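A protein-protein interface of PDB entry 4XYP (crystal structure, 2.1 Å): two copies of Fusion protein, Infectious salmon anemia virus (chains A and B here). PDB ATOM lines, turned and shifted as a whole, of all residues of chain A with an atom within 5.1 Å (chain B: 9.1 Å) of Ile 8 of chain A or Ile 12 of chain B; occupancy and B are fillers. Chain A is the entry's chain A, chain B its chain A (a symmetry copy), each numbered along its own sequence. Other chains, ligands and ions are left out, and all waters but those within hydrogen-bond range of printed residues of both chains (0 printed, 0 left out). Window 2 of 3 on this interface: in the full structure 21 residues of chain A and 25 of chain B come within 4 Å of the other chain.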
ATOM      1  N   GLU A   3      -2.363 -11.119   8.734  1.00  0.00           N
ATOM      2  CA  GLU A   3      -1.223 -10.208   8.810  1.00  0.00           C
ATOM      3  C   GLU A   3      -1.609  -8.744   8.549  1.00  0.00           C
ATOM      4  O   GLU A   3      -0.932  -7.809   9.019  1.00  0.00           O
ATOM      5  CB  GLU A   3      -0.139 -10.644   7.822  1.00  0.00           C
ATOM      6  N   LYS A   4      -2.684  -8.527   7.803  1.00  0.00           N
ATOM      7  CA  LYS A   4      -3.158  -7.168   7.619  1.00  0.00           C
ATOM      8  C   LYS A   4      -3.746  -6.711   8.969  1.00  0.00           C
ATOM      9  O   LYS A   4      -3.452  -5.619   9.458  1.00  0.00           O
ATOM     10  CB  LYS A   4      -4.175  -7.076   6.486  1.00  0.00           C
ATOM     11  N   LEU A   5      -4.523  -7.573   9.600  1.00  0.00           N
ATOM     12  CA  LEU A   5      -5.143  -7.225  10.870  1.00  0.00           C
ATOM     13  C   LEU A   5      -4.110  -7.083  11.948  1.00  0.00           C
ATOM     14  O   LEU A   5      -4.231  -6.197  12.796  1.00  0.00           O
ATOM     15  CB  LEU A   5      -6.172  -8.255  11.296  1.00  0.00           C
ATOM     16  CG  LEU A   5      -7.379  -8.371  10.375  1.00  0.00           C
ATOM     17  CD1 LEU A   5      -8.225  -9.524  10.825  1.00  0.00           C
ATOM     18  CD2 LEU A   5      -8.209  -7.115  10.401  1.00  0.00           C
ATOM     19  N   ASN A   6      -3.085  -7.935  11.931  1.00  0.00           N
ATOM     20  CA  ASN A   6      -2.033  -7.830  12.926  1.00  0.00           C
ATOM     21  C   ASN A   6      -1.221  -6.559  12.704  1.00  0.00           C
ATOM     22  O   ASN A   6      -0.793  -5.918  13.660  1.00  0.00           O
ATOM     23  CB  ASN A   6      -1.133  -9.057  12.936  1.00  0.00           C
ATOM     24  CG  ASN A   6      -1.041  -9.687  14.311  1.00  0.00           C
ATOM     25  OD1 ASN A   6      -2.061 -10.006  14.934  1.00  0.00           O
ATOM     26  ND2 ASN A   6       0.178  -9.832  14.814  1.00  0.00           N
ATOM     27  N   GLY A   7      -1.045  -6.167  11.446  1.00  0.00           N
ATOM     28  CA  GLY A   7      -0.333  -4.929  11.144  1.00  0.00           C
ATOM     29  C   GLY A   7      -1.110  -3.728  11.673  1.00  0.00           C
ATOM     30  O   GLY A   7      -0.545  -2.795  12.246  1.00  0.00           O
ATOM     31  N   ILE A   8      -2.427  -3.783  11.520  1.00  0.00           N
ATOM     32  CA  ILE A   8      -3.293  -2.720  11.979  1.00  0.00           C
ATOM     33  C   ILE A   8      -3.268  -2.581  13.507  1.00  0.00           C
ATOM     34  O   ILE A   8      -3.124  -1.471  14.041  1.00  0.00           O
ATOM     35  CB  ILE A   8      -4.689  -2.964  11.493  1.00  0.00           C
ATOM     36  CG1 ILE A   8      -4.691  -2.698   9.980  1.00  0.00           C
ATOM     37  CG2 ILE A   8      -5.701  -2.046  12.208  1.00  0.00           C
ATOM     38  CD1 ILE A   8      -5.970  -3.040   9.267  1.00  0.00           C
ATOM     39  N   ILE A   9      -3.413  -3.704  14.196  1.00  0.00           N
ATOM     40  CA  ILE A   9      -3.367  -3.721  15.642  1.00  0.00           C
ATOM     41  C   ILE A   9      -2.067  -3.137  16.144  1.00  0.00           C
ATOM     42  O   ILE A   9      -2.074  -2.384  17.107  1.00  0.00           O
ATOM     43  CB  ILE A   9      -3.565  -5.137  16.179  1.00  0.00           C
ATOM     44  CG1 ILE A   9      -5.010  -5.547  15.919  1.00  0.00           C
ATOM     45  CG2 ILE A   9      -3.251  -5.206  17.690  1.00  0.00           C
ATOM     46  CD1 ILE A   9      -5.284  -7.050  16.041  1.00  0.00           C
ATOM     47  N   ASP A  10      -0.962  -3.456  15.487  1.00  0.00           N
ATOM     48  CA  ASP A  10       0.337  -2.909  15.849  1.00  0.00           C
ATOM     49  C   ASP A  10       0.411  -1.394  15.728  1.00  0.00           C
ATOM     50  O   ASP A  10       0.999  -0.733  16.598  1.00  0.00           O
ATOM     51  CB  ASP A  10       1.430  -3.528  14.996  1.00  0.00           C
ATOM     52  CG  ASP A  10       1.708  -4.970  15.375  1.00  0.00           C
ATOM     53  OD1 ASP A  10       1.387  -5.345  16.528  1.00  0.00           O
ATOM     54  OD2 ASP A  10       2.253  -5.725  14.532  1.00  0.00           O
ATOM     55  N   GLN A  11      -0.173  -0.835  14.665  1.00  0.00           N
ATOM     56  CA  GLN A  11      -0.226   0.632  14.532  1.00  0.00           C
ATOM     57  C   GLN A  11      -1.109   1.257  15.612  1.00  0.00           C
ATOM     58  O   GLN A  11      -0.765   2.300  16.180  1.00  0.00           O
ATOM     59  CB  GLN A  11      -0.729   1.060  13.137  1.00  0.00           C
ATOM     60  CG  GLN A  11       0.194   0.639  12.025  1.00  0.00           C
ATOM     61  CD  GLN A  11       1.498   1.348  12.104  1.00  0.00           C
ATOM     62  OE1 GLN A  11       1.545   2.585  12.041  1.00  0.00           O
ATOM     63  NE2 GLN A  11       2.578   0.592  12.253  1.00  0.00           N
ATOM     64  N   ILE A  12      -2.213   0.607  15.952  1.00  0.00           N
ATOM     65  CA  ILE A  12      -3.033   1.137  17.050  1.00  0.00           C
ATOM     66  C   ILE A  12      -2.218   1.187  18.339  1.00  0.00           C
ATOM     67  O   ILE A  12      -2.220   2.198  19.024  1.00  0.00           O
ATOM     68  CB  ILE A  12      -4.331   0.320  17.282  1.00  0.00           C
ATOM     69  CG1 ILE A  12      -5.256   0.457  16.075  1.00  0.00           C
ATOM     70  CG2 ILE A  12      -5.080   0.775  18.588  1.00  0.00           C
ATOM     71  CD1 ILE A  12      -6.331  -0.641  16.023  1.00  0.00           C
ATOM     72  N   VAL A  15       0.305   4.081  18.077  1.00  0.00           N
ATOM     73  CA  VAL A  15      -0.339   5.367  18.306  1.00  0.00           C
ATOM     74  C   VAL A  15      -0.644   5.573  19.794  1.00  0.00           C
ATOM     75  O   VAL A  15      -0.439   6.673  20.360  1.00  0.00           O
ATOM     76  CB  VAL A  15      -1.644   5.511  17.502  1.00  0.00           C
ATOM     77  CG1 VAL A  15      -2.349   6.787  17.886  1.00  0.00           C
ATOM     78  CG2 VAL A  15      -1.363   5.551  16.001  1.00  0.00           C
ATOM     79  N   VAL B   1     -13.947  -6.147   2.014  1.00  0.00           N
ATOM     80  CA  VAL B   1     -12.730  -6.595   2.698  1.00  0.00           C
ATOM     81  C   VAL B   1     -11.673  -5.503   2.707  1.00  0.00           C
ATOM     82  O   VAL B   1     -11.377  -4.912   3.756  1.00  0.00           O
ATOM     83  CB  VAL B   1     -12.123  -7.843   2.033  1.00  0.00           C
ATOM     84  N   LYS B   2     -11.117  -5.241   1.523  1.00  0.00           N
ATOM     85  CA  LYS B   2     -10.087  -4.224   1.335  1.00  0.00           C
ATOM     86  C   LYS B   2     -10.567  -2.850   1.789  1.00  0.00           C
ATOM     87  O   LYS B   2      -9.782  -2.063   2.316  1.00  0.00           O
ATOM     88  CB  LYS B   2      -9.651  -4.163  -0.141  1.00  0.00           C
ATOM     89  N   LYS B   4     -13.064  -2.212   4.079  1.00  0.00           N
ATOM     90  CA  LYS B   4     -13.302  -2.133   5.510  1.00  0.00           C
ATOM     91  C   LYS B   4     -11.945  -1.832   6.175  1.00  0.00           C
ATOM     92  O   LYS B   4     -11.830  -0.945   7.022  1.00  0.00           O
ATOM     93  CB  LYS B   4     -13.936  -3.413   6.045  1.00  0.00           C
ATOM     94  N   LEU B   5     -10.906  -2.524   5.742  1.00  0.00           N
ATOM     95  CA  LEU B   5      -9.586  -2.327   6.324  1.00  0.00           C
ATOM     96  C   LEU B   5      -9.052  -0.965   5.991  1.00  0.00           C
ATOM     97  O   LEU B   5      -8.412  -0.338   6.837  1.00  0.00           O
ATOM     98  CB  LEU B   5      -8.599  -3.378   5.854  1.00  0.00           C
ATOM     99  CG  LEU B   5      -8.928  -4.801   6.286  1.00  0.00           C
ATOM    100  CD1 LEU B   5      -7.969  -5.745   5.624  1.00  0.00           C
ATOM    101  CD2 LEU B   5      -8.818  -4.958   7.780  1.00  0.00           C
ATOM    102  N   ASN B   6      -9.310  -0.486   4.774  1.00  0.00           N
ATOM    103  CA  ASN B   6      -8.851   0.839   4.400  1.00  0.00           C
ATOM    104  C   ASN B   6      -9.615   1.902   5.182  1.00  0.00           C
ATOM    105  O   ASN B   6      -9.049   2.922   5.565  1.00  0.00           O
ATOM    106  CB  ASN B   6      -8.964   1.079   2.902  1.00  0.00           C
ATOM    107  CG  ASN B   6      -7.643   1.506   2.292  1.00  0.00           C
ATOM    108  OD1 ASN B   6      -6.620   0.831   2.454  1.00  0.00           O
ATOM    109  ND2 ASN B   6      -7.646   2.651   1.621  1.00  0.00           N
ATOM    110  N   GLY B   7     -10.890   1.648   5.461  1.00  0.00           N
ATOM    111  CA  GLY B   7     -11.680   2.582   6.257  1.00  0.00           C
ATOM    112  C   GLY B   7     -11.127   2.666   7.676  1.00  0.00           C
ATOM    113  O   GLY B   7     -11.014   3.745   8.261  1.00  0.00           O
ATOM    114  N   ILE B   8     -10.734   1.516   8.210  1.00  0.00           N
ATOM    115  CA  ILE B   8     -10.182   1.444   9.544  1.00  0.00           C
ATOM    116  C   ILE B   8      -8.846   2.191   9.653  1.00  0.00           C
ATOM    117  O   ILE B   8      -8.636   2.983  10.583  1.00  0.00           O
ATOM    118  CB  ILE B   8     -10.021   0.010   9.944  1.00  0.00           C
ATOM    119  CG1 ILE B   8     -11.430  -0.549  10.188  1.00  0.00           C
ATOM    120  CG2 ILE B   8      -9.153  -0.125  11.212  1.00  0.00           C
ATOM    121  CD1 ILE B   8     -11.500  -2.030  10.449  1.00  0.00           C
ATOM    122  N   ILE B   9      -7.955   1.929   8.707  1.00  0.00           N
ATOM    123  CA  ILE B   9      -6.671   2.594   8.667  1.00  0.00           C
ATOM    124  C   ILE B   9      -6.844   4.095   8.614  1.00  0.00           C
ATOM    125  O   ILE B   9      -6.121   4.812   9.290  1.00  0.00           O
ATOM    126  CB  ILE B   9      -5.840   2.107   7.483  1.00  0.00           C
ATOM    127  CG1 ILE B   9      -5.423   0.666   7.754  1.00  0.00           C
ATOM    128  CG2 ILE B   9      -4.593   2.995   7.276  1.00  0.00           C
ATOM    129  CD1 ILE B   9      -4.918  -0.101   6.527  1.00  0.00           C
ATOM    130  N   ASP B  10      -7.810   4.568   7.842  1.00  0.00           N
ATOM    131  CA  ASP B  10      -8.104   5.992   7.757  1.00  0.00           C
ATOM    132  C   ASP B  10      -8.531   6.601   9.084  1.00  0.00           C
ATOM    133  O   ASP B  10      -8.108   7.720   9.415  1.00  0.00           O
ATOM    134  CB  ASP B  10      -9.183   6.250   6.722  1.00  0.00           C
ATOM    135  CG  ASP B  10      -8.676   6.066   5.305  1.00  0.00           C
ATOM    136  OD1 ASP B  10      -7.442   6.164   5.107  1.00  0.00           O
ATOM    137  OD2 ASP B  10      -9.505   5.834   4.389  1.00  0.00           O
ATOM    138  N   GLN B  11      -9.362   5.888   9.846  1.00  0.00           N
ATOM    139  CA  GLN B  11      -9.742   6.371  11.188  1.00  0.00           C
ATOM    140  C   GLN B  11      -8.542   6.382  12.134  1.00  0.00           C
ATOM    141  O   GLN B  11      -8.367   7.325  12.917  1.00  0.00           O
ATOM    142  CB  GLN B  11     -10.878   5.523  11.798  1.00  0.00           C
ATOM    143  CG  GLN B  11     -12.161   5.612  11.016  1.00  0.00           C
ATOM    144  CD  GLN B  11     -12.741   6.978  11.076  1.00  0.00           C
ATOM    145  OE1 GLN B  11     -13.053   7.482  12.164  1.00  0.00           O
ATOM    146  NE2 GLN B  11     -12.890   7.613   9.919  1.00  0.00           N
ATOM    147  N   ILE B  12      -7.676   5.384  12.038  1.00  0.00           N
ATOM    148  CA  ILE B  12      -6.466   5.416  12.872  1.00  0.00           C
ATOM    149  C   ILE B  12      -5.640   6.659  12.552  1.00  0.00           C
ATOM    150  O   ILE B  12      -5.218   7.361  13.458  1.00  0.00           O
ATOM    151  CB  ILE B  12      -5.590   4.147  12.713  1.00  0.00           C
ATOM    152  CG1 ILE B  12      -6.335   2.927  13.248  1.00  0.00           C
ATOM    153  CG2 ILE B  12      -4.206   4.299  13.448  1.00  0.00           C
ATOM    154  CD1 ILE B  12      -5.747   1.602  12.738  1.00  0.00           C
ATOM    155  N   ASN B  13      -5.437   6.958  11.278  1.00  0.00           N
ATOM    156  CA  ASN B  13      -4.737   8.186  10.898  1.00  0.00           C
ATOM    157  C   ASN B  13      -5.439   9.442  11.388  1.00  0.00           C
ATOM    158  O   ASN B  13      -4.771  10.334  11.881  1.00  0.00           O
ATOM    159  CB  ASN B  13      -4.551   8.246   9.384  1.00  0.00           C
ATOM    160  CG  ASN B  13      -3.640   7.182   8.912  1.00  0.00           C
ATOM    161  OD1 ASN B  13      -2.773   6.761   9.664  1.00  0.00           O
ATOM    162  ND2 ASN B  13      -3.843   6.693   7.698  1.00  0.00           N
ATOM    163  N   LYS B  14      -6.770   9.514  11.295  1.00  0.00           N
ATOM    164  CA  LYS B  14      -7.456  10.694  11.816  1.00  0.00           C
ATOM    165  C   LYS B  14      -7.282  10.826  13.302  1.00  0.00           C
ATOM    166  O   LYS B  14      -7.006  11.915  13.799  1.00  0.00           O
ATOM    167  CB  LYS B  14      -8.930  10.674  11.489  1.00  0.00           C
ATOM    168  CG  LYS B  14      -9.186  10.960  10.038  1.00  0.00           C
ATOM    169  CD  LYS B  14     -10.689  11.146   9.816  1.00  0.00           C
ATOM    170  CE  LYS B  14     -11.070  11.131   8.357  1.00  0.00           C
ATOM    171  NZ  LYS B  14     -11.511   9.770   7.952  1.00  0.00           N
ATOM    172  N   VAL B  15      -7.426   9.728  14.034  1.00  0.00           N
ATOM    173  CA  VAL B  15      -7.213   9.822  15.473  1.00  0.00           C
ATOM    174  C   VAL B  15      -5.794  10.312  15.787  1.00  0.00           C
ATOM    175  O   VAL B  15      -5.577  11.164  16.680  1.00  0.00           O
ATOM    176  CB  VAL B  15      -7.446   8.477  16.180  1.00  0.00           C
ATOM    177  CG1 VAL B  15      -7.067   8.585  17.636  1.00  0.00           C
ATOM    178  CG2 VAL B  15      -8.914   8.060  16.097  1.00  0.00           C
ATOM    179  N   ASN B  16      -4.817   9.751  15.090  1.00  0.00           N
ATOM    180  CA  ASN B  16      -3.423  10.130  15.330  1.00  0.00           C
ATOM    181  C   ASN B  16      -3.230  11.605  15.068  1.00  0.00           C
ATOM    182  O   ASN B  16      -2.738  12.337  15.928  1.00  0.00           O
ATOM    183  CB  ASN B  16      -2.495   9.296  14.452  1.00  0.00           C
ATOM    184  CG  ASN B  16      -1.044   9.338  14.925  1.00  0.00           C
ATOM    185  OD1 ASN B  16      -0.658  10.193  15.719  1.00  0.00           O
ATOM    186  ND2 ASN B  16      -0.240   8.425  14.418  1.00  0.00           N
ATOM    187  N   LEU B  17      -3.683  12.078  13.914  1.00  0.00           N
ATOM    188  CA  LEU B  17      -3.471  13.479  13.556  1.00  0.00           C
ATOM    189  C   LEU B  17      -4.188  14.436  14.477  1.00  0.00           C
ATOM    190  O   LEU B  17      -3.622  15.444  14.913  1.00  0.00           O
ATOM    191  CB  LEU B  17      -3.960  13.762  12.148  1.00  0.00           C
ATOM    192  CG  LEU B  17      -3.081  13.221  11.038  1.00  0.00           C
ATOM    193  CD1 LEU B  17      -3.841  13.251   9.726  1.00  0.00           C
ATOM    194  CD2 LEU B  17      -1.836  14.074  10.973  1.00  0.00           C
ATOM    195  N   LEU B  18      -5.448  14.135  14.779  1.00  0.00           N
ATOM    196  CA  LEU B  18      -6.224  15.064  15.574  1.00  0.00           C
ATOM    197  C   LEU B  18      -5.634  15.187  16.955  1.00  0.00           C
ATOM    198  O   LEU B  18      -5.448  16.293  17.448  1.00  0.00           O
ATOM    199  CB  LEU B  18      -7.682  14.633  15.648  1.00  0.00           C
ATOM    200  CG  LEU B  18      -8.340  14.674  14.260  1.00  0.00           C
ATOM    201  CD1 LEU B  18      -9.715  13.985  14.294  1.00  0.00           C
ATOM    202  CD2 LEU B  18      -8.497  16.105  13.804  1.00  0.00           C
ATOM    203  N   LEU B  19      -5.325  14.058  17.580  1.00  0.00           N
ATOM    204  CA  LEU B  19      -4.873  14.093  18.955  1.00  0.00           C
ATOM    205  C   LEU B  19      -3.474  14.669  19.046  1.00  0.00           C
ATOM    206  O   LEU B  19      -3.175  15.431  19.969  1.00  0.00           O
ATOM    207  CB  LEU B  19      -4.918  12.693  19.587  1.00  0.00           C
ATOM    208  CG  LEU B  19      -6.347  12.144  19.754  1.00  0.00           C
ATOM    209  CD1 LEU B  19      -6.333  10.955  20.649  1.00  0.00           C
ATOM    210  CD2 LEU B  19      -7.367  13.162  20.268  1.00  0.00           C
ATOM    211  N   GLU B  20      -2.622  14.328  18.085  1.00  0.00           N
ATOM    212  CA  GLU B  20      -1.260  14.863  18.076  1.00  0.00           C
ATOM    213  C   GLU B  20      -1.293  16.386  17.954  1.00  0.00           C
ATOM    214  O   GLU B  20      -0.462  17.094  18.530  1.00  0.00           O
ATOM    215  CB  GLU B  20      -0.457  14.252  16.932  1.00  0.00           C
ATOM    216  CG  GLU B  20       0.943  14.811  16.794  1.00  0.00           C
ATOM    217  CD  GLU B  20       1.802  14.524  18.006  1.00  0.00           C
ATOM    218  OE1 GLU B  20       1.983  13.320  18.310  1.00  0.00           O
ATOM    219  OE2 GLU B  20       2.288  15.496  18.646  1.00  0.00           O
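Ile 12 of chain B touches two residues of chain A. Printed residues of chain A within 4 Å of Leu 5 of chain B: Leu 5 and Ile 8. Of the printed residues of chain B, Ile 12 of chain A touches Ile 12. Of the printed residues of chain A, Asn 16 of chain B touches Val 15. Of the printed residues of chain B, Val 15 of chain A touches Asn 16. Of the printed residues of chain B, Leu 5 of chain A touches Leu 5 (3.4 Å).
CD2 of Leu 5 of chain B touches CD2 of Leu 5 of chain A (3.4 Å). Ile 8 of chain A touches Leu 5 of chain B (CD1 to CD2, 3.7 Å). Ile 12 of chain B touches Ile 8 of chain A (CD1 to CG2, 3.7 Å). Ile 12 of chain B touches Ile 12 of chain A. Val 15 of chain A touches Asn 16 of chain B (CG2 to ND2, 3.5 Å).
Printed residues of chain A that touch a printed residue of chain B: Leu 5, Ile 8, Ile 12 and Val 15. Hydrophobic or aromatic side chains of chain A that line the printed part of chain B: Leu 5, Ile 8, Ile 12 and Val 15. Hydrophobic or aromatic side chains of chain B within 4 Å of the printed part of chain A: Leu 5 and Ile 12.
Leu 5 of chain A touches its own counterpart, Leu 5 of chain B. Ile 8 of chain A touches Leu 5 of chain B, but with the chains exchanged Leu 5 of chain A does not touch Ile 8 of chain B (6.1 Å). Ile 8 of chain A touches Ile 12 of chain B, but with the chains exchanged Ile 12 of chain A does not touch Ile 8 of chain B (5.6 Å). Ile 12 of chain B touches its own counterpart, Ile 12 of chain A. 10 positions are printed for both chains.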
